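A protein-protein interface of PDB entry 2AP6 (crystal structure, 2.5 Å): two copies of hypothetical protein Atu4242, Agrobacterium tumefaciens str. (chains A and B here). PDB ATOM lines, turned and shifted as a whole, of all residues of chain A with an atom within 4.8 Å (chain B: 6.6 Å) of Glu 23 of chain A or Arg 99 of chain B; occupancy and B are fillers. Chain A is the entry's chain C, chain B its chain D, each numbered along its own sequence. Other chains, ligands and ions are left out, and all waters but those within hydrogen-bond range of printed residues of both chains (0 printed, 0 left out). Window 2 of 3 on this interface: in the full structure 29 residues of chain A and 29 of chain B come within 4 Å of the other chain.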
ATOM      1  N   LEU A  19     -24.088  -2.465   9.493  1.00  0.00           N
ATOM      2  CA  LEU A  19     -25.208  -1.556   9.305  1.00  0.00           C
ATOM      3  C   LEU A  19     -25.293  -1.018   7.882  1.00  0.00           C
ATOM      4  O   LEU A  19     -26.386  -0.744   7.379  1.00  0.00           O
ATOM      5  CB  LEU A  19     -25.101  -0.397  10.290  1.00  0.00           C
ATOM      6  CG  LEU A  19     -25.317  -0.704  11.773  1.00  0.00           C
ATOM      7  CD1 LEU A  19     -24.980   0.542  12.573  1.00  0.00           C
ATOM      8  CD2 LEU A  19     -26.753  -1.147  12.031  1.00  0.00           C
ATOM      9  N   LYS A  20     -24.144  -0.863   7.227  1.00  0.00           N
ATOM     10  CA  LYS A  20     -24.149  -0.354   5.856  1.00  0.00           C
ATOM     11  C   LYS A  20     -24.747  -1.339   4.862  1.00  0.00           C
ATOM     12  O   LYS A  20     -25.602  -0.972   4.066  1.00  0.00           O
ATOM     13  CB  LYS A  20     -22.738   0.000   5.379  1.00  0.00           C
ATOM     14  CG  LYS A  20     -22.787   0.773   4.071  1.00  0.00           C
ATOM     15  CD  LYS A  20     -21.466   0.842   3.351  1.00  0.00           C
ATOM     16  CE  LYS A  20     -21.658   1.549   2.029  1.00  0.00           C
ATOM     17  NZ  LYS A  20     -20.474   1.362   1.163  1.00  0.00           N
ATOM     18  N   VAL A  21     -24.280  -2.587   4.906  1.00  0.00           N
ATOM     19  CA  VAL A  21     -24.758  -3.622   4.001  1.00  0.00           C
ATOM     20  C   VAL A  21     -26.199  -4.038   4.297  1.00  0.00           C
ATOM     21  O   VAL A  21     -26.939  -4.412   3.396  1.00  0.00           O
ATOM     22  CB  VAL A  21     -23.832  -4.857   4.041  1.00  0.00           C
ATOM     23  CG1 VAL A  21     -23.945  -5.557   5.400  1.00  0.00           C
ATOM     24  CG2 VAL A  21     -24.179  -5.803   2.880  1.00  0.00           C
ATOM     25  N   VAL A  22     -26.598  -3.969   5.562  1.00  0.00           N
ATOM     26  CA  VAL A  22     -27.963  -4.312   5.946  1.00  0.00           C
ATOM     27  C   VAL A  22     -28.892  -3.252   5.344  1.00  0.00           C
ATOM     28  O   VAL A  22     -29.902  -3.578   4.727  1.00  0.00           O
ATOM     29  CB  VAL A  22     -28.109  -4.345   7.493  1.00  0.00           C
ATOM     30  CG1 VAL A  22     -29.575  -4.376   7.893  1.00  0.00           C
ATOM     31  CG2 VAL A  22     -27.406  -5.559   8.035  1.00  0.00           C
ATOM     32  N   GLU A  23     -28.523  -1.984   5.516  1.00  0.00           N
ATOM     33  CA  GLU A  23     -29.294  -0.877   4.981  1.00  0.00           C
ATOM     34  C   GLU A  23     -29.352  -0.938   3.462  1.00  0.00           C
ATOM     35  O   GLU A  23     -30.412  -0.766   2.861  1.00  0.00           O
ATOM     36  CB  GLU A  23     -28.661   0.449   5.391  1.00  0.00           C
ATOM     37  CG  GLU A  23     -29.151   1.634   4.584  1.00  0.00           C
ATOM     38  CD  GLU A  23     -28.765   2.948   5.201  1.00  0.00           C
ATOM     39  OE1 GLU A  23     -27.695   3.022   5.836  1.00  0.00           O
ATOM     40  OE2 GLU A  23     -29.534   3.912   5.043  1.00  0.00           O
ATOM     41  N   ASP A  24     -28.201  -1.181   2.846  1.00  0.00           N
ATOM     42  CA  ASP A  24     -28.094  -1.230   1.396  1.00  0.00           C
ATOM     43  C   ASP A  24     -28.658  -2.458   0.705  1.00  0.00           C
ATOM     44  O   ASP A  24     -29.147  -2.362  -0.423  1.00  0.00           O
ATOM     45  CB  ASP A  24     -26.631  -1.111   0.961  1.00  0.00           C
ATOM     46  CG  ASP A  24     -26.033   0.236   1.270  1.00  0.00           C
ATOM     47  OD1 ASP A  24     -26.776   1.242   1.301  1.00  0.00           O
ATOM     48  OD2 ASP A  24     -24.805   0.280   1.459  1.00  0.00           O
ATOM     49  N   GLU A  25     -28.595  -3.612   1.363  1.00  0.00           N
ATOM     50  CA  GLU A  25     -29.053  -4.837   0.721  1.00  0.00           C
ATOM     51  C   GLU A  25     -29.941  -5.817   1.476  1.00  0.00           C
ATOM     52  O   GLU A  25     -30.479  -6.724   0.867  1.00  0.00           O
ATOM     53  CB  GLU A  25     -27.833  -5.610   0.229  1.00  0.00           C
ATOM     54  CG  GLU A  25     -26.817  -4.763  -0.498  1.00  0.00           C
ATOM     55  CD  GLU A  25     -25.685  -5.598  -1.032  1.00  0.00           C
ATOM     56  OE1 GLU A  25     -24.790  -5.058  -1.716  1.00  0.00           O
ATOM     57  OE2 GLU A  25     -25.700  -6.817  -0.759  1.00  0.00           O
ATOM     58  N   ILE A  27     -32.232  -5.075   4.746  1.00  0.00           N
ATOM     59  CA  ILE A  27     -33.416  -4.628   5.462  1.00  0.00           C
ATOM     60  C   ILE A  27     -34.713  -4.561   4.641  1.00  0.00           C
ATOM     61  O   ILE A  27     -35.772  -4.973   5.133  1.00  0.00           O
ATOM     62  CB  ILE A  27     -33.157  -3.269   6.159  1.00  0.00           C
ATOM     63  CG1 ILE A  27     -34.204  -3.033   7.245  1.00  0.00           C
ATOM     64  CG2 ILE A  27     -33.166  -2.144   5.132  1.00  0.00           C
ATOM     65  CD1 ILE A  27     -34.162  -4.049   8.350  1.00  0.00           C
ATOM     66  N   PRO B  97     -30.360   4.199  17.256  1.00  0.00           N
ATOM     67  CA  PRO B  97     -31.133   3.613  16.164  1.00  0.00           C
ATOM     68  C   PRO B  97     -30.371   3.597  14.865  1.00  0.00           C
ATOM     69  O   PRO B  97     -29.618   4.531  14.563  1.00  0.00           O
ATOM     70  CB  PRO B  97     -32.345   4.523  16.090  1.00  0.00           C
ATOM     71  CG  PRO B  97     -31.699   5.881  16.322  1.00  0.00           C
ATOM     72  CD  PRO B  97     -30.761   5.601  17.491  1.00  0.00           C
ATOM     73  N   ALA B  98     -30.562   2.526  14.100  1.00  0.00           N
ATOM     74  CA  ALA B  98     -29.934   2.412  12.791  1.00  0.00           C
ATOM     75  C   ALA B  98     -30.673   3.418  11.913  1.00  0.00           C
ATOM     76  O   ALA B  98     -31.812   3.776  12.199  1.00  0.00           O
ATOM     77  CB  ALA B  98     -30.108   0.998  12.245  1.00  0.00           C
ATOM     78  N   ARG B  99     -30.031   3.883  10.854  1.00  0.00           N
ATOM     79  CA  ARG B  99     -30.658   4.859   9.967  1.00  0.00           C
ATOM     80  C   ARG B  99     -31.988   4.337   9.433  1.00  0.00           C
ATOM     81  O   ARG B  99     -32.896   5.105   9.107  1.00  0.00           O
ATOM     82  CB  ARG B  99     -29.738   5.168   8.788  1.00  0.00           C
ATOM     83  CG  ARG B  99     -28.463   5.908   9.135  1.00  0.00           C
ATOM     84  CD  ARG B  99     -27.394   5.639   8.064  1.00  0.00           C
ATOM     85  NE  ARG B  99     -27.958   5.818   6.733  1.00  0.00           N
ATOM     86  CZ  ARG B  99     -28.079   6.995   6.130  1.00  0.00           C
ATOM     87  NH1 ARG B  99     -27.649   8.092   6.734  1.00  0.00           N
ATOM     88  NH2 ARG B  99     -28.693   7.080   4.955  1.00  0.00           N
ATOM     89  N   PHE B 100     -32.095   3.019   9.351  1.00  0.00           N
ATOM     90  CA  PHE B 100     -33.287   2.382   8.821  1.00  0.00           C
ATOM     91  C   PHE B 100     -34.222   1.876   9.893  1.00  0.00           C
ATOM     92  O   PHE B 100     -35.059   1.010   9.636  1.00  0.00           O
ATOM     93  CB  PHE B 100     -32.879   1.234   7.891  1.00  0.00           C
ATOM     94  CG  PHE B 100     -31.847   0.323   8.471  1.00  0.00           C
ATOM     95  CD1 PHE B 100     -32.220  -0.742   9.280  1.00  0.00           C
ATOM     96  CD2 PHE B 100     -30.502   0.524   8.196  1.00  0.00           C
ATOM     97  CE1 PHE B 100     -31.264  -1.604   9.809  1.00  0.00           C
ATOM     98  CE2 PHE B 100     -29.536  -0.327   8.719  1.00  0.00           C
ATOM     99  CZ  PHE B 100     -29.922  -1.402   9.533  1.00  0.00           C
ATOM    100  N   SER B 101     -34.076   2.419  11.094  1.00  0.00           N
ATOM    101  CA  SER B 101     -34.917   2.033  12.213  1.00  0.00           C
ATOM    102  C   SER B 101     -36.146   2.918  12.233  1.00  0.00           C
ATOM    103  O   SER B 101     -36.054   4.111  11.991  1.00  0.00           O
ATOM    104  CB  SER B 101     -34.163   2.190  13.528  1.00  0.00           C
ATOM    105  OG  SER B 101     -34.962   1.768  14.623  1.00  0.00           O
ATOM    106  N   PRO B 102     -37.324   2.335  12.497  1.00  0.00           N
ATOM    107  CA  PRO B 102     -38.536   3.167  12.532  1.00  0.00           C
ATOM    108  C   PRO B 102     -38.274   4.139  13.675  1.00  0.00           C
ATOM    109  O   PRO B 102     -38.545   5.336  13.586  1.00  0.00           O
ATOM    110  CB  PRO B 102     -39.642   2.170  12.882  1.00  0.00           C
ATOM    111  CG  PRO B 102     -39.061   0.815  12.502  1.00  0.00           C
ATOM    112  CD  PRO B 102     -37.614   0.943  12.884  1.00  0.00           C
ATOM    113  N   MET B 104     -36.173   6.375  15.695  1.00  0.00           N
ATOM    114  CA  MET B 104     -35.025   7.233  15.414  1.00  0.00           C
ATOM    115  C   MET B 104     -34.788   8.290  16.481  1.00  0.00           C
ATOM    116  O   MET B 104     -35.478   8.243  17.539  1.00  0.00           O
ATOM    117  CB  MET B 104     -35.199   7.905  14.045  1.00  0.00           C
ATOM    118  CG  MET B 104     -35.056   6.932  12.859  1.00  0.00           C
ATOM    119  SD  MET B 104     -33.183   6.302  12.491  1.00  0.00           S
ATOM    120  CE  MET B 104     -32.604   7.894  11.390  1.00  0.00           C
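Among the printed residues, pairs that only touch across the chains: Leu 19 of chain A with Ala 98 of chain B (3.99 Å), Leu 19 of chain A with Phe 100 of chain B (3.4 Å), Val 22 of chain A with Phe 100 of chain B (3.4 Å), Glu 23 of chain A with Phe 100 of chain B (3.4 Å) and Ile 27 of chain A with Phe 100 of chain B (3.7 Å).
Of the 7 printed residues of chain B, 3 touch a printed residue of chain A. Hydrophobic or aromatic side chains of chain B within 4 Å of the printed part of chain A: Ala 98 and Phe 100. Of the 8 printed residues of chain A, 4 touch a printed residue of chain B. Printed residues of chain A that touch a printed residue of chain B: Leu 19, Val 22, Glu 23 and Ile 27. Hydrophobic or aromatic side chains of chain A within 4 Å of the printed part of chain B: Leu 19, Val 22 and Ile 27. Among the printed residues, Asp or Glu carboxylates within 4 Å of a Lys or Arg side-chain nitrogen of the other chain: Glu 23 of chain A with Arg 99 of chain B (2.9 Å).
No position is printed for both chains.
The guanidinium group (NE) of Arg 99 of chain B is in salt-bridge range of the side-chain carboxylate (OE1) of Glu 23 of chain A.
Glu 23 of chain A touches just these residues of chain B: Arg 99 and Phe 100. Of chain A, only Glu 23 comes within 4 Å of Arg 99 of chain B. Of the printed residues of chain A, Ala 98 of chain B touches Leu 19. Printed residues of chain B within 4 Å of Ile 27 of chain A: Phe 100. Val 21 of chain A touches none of the printed residues of chain B. The nearest printed residue of chain A that does not touch Arg 99 of chain B is Leu 19 of chain A (6.1 Å).
N of Ile 27 of chain A lies within hydrogen-bond range of O of Val 22 of chain A (2.8 Å).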
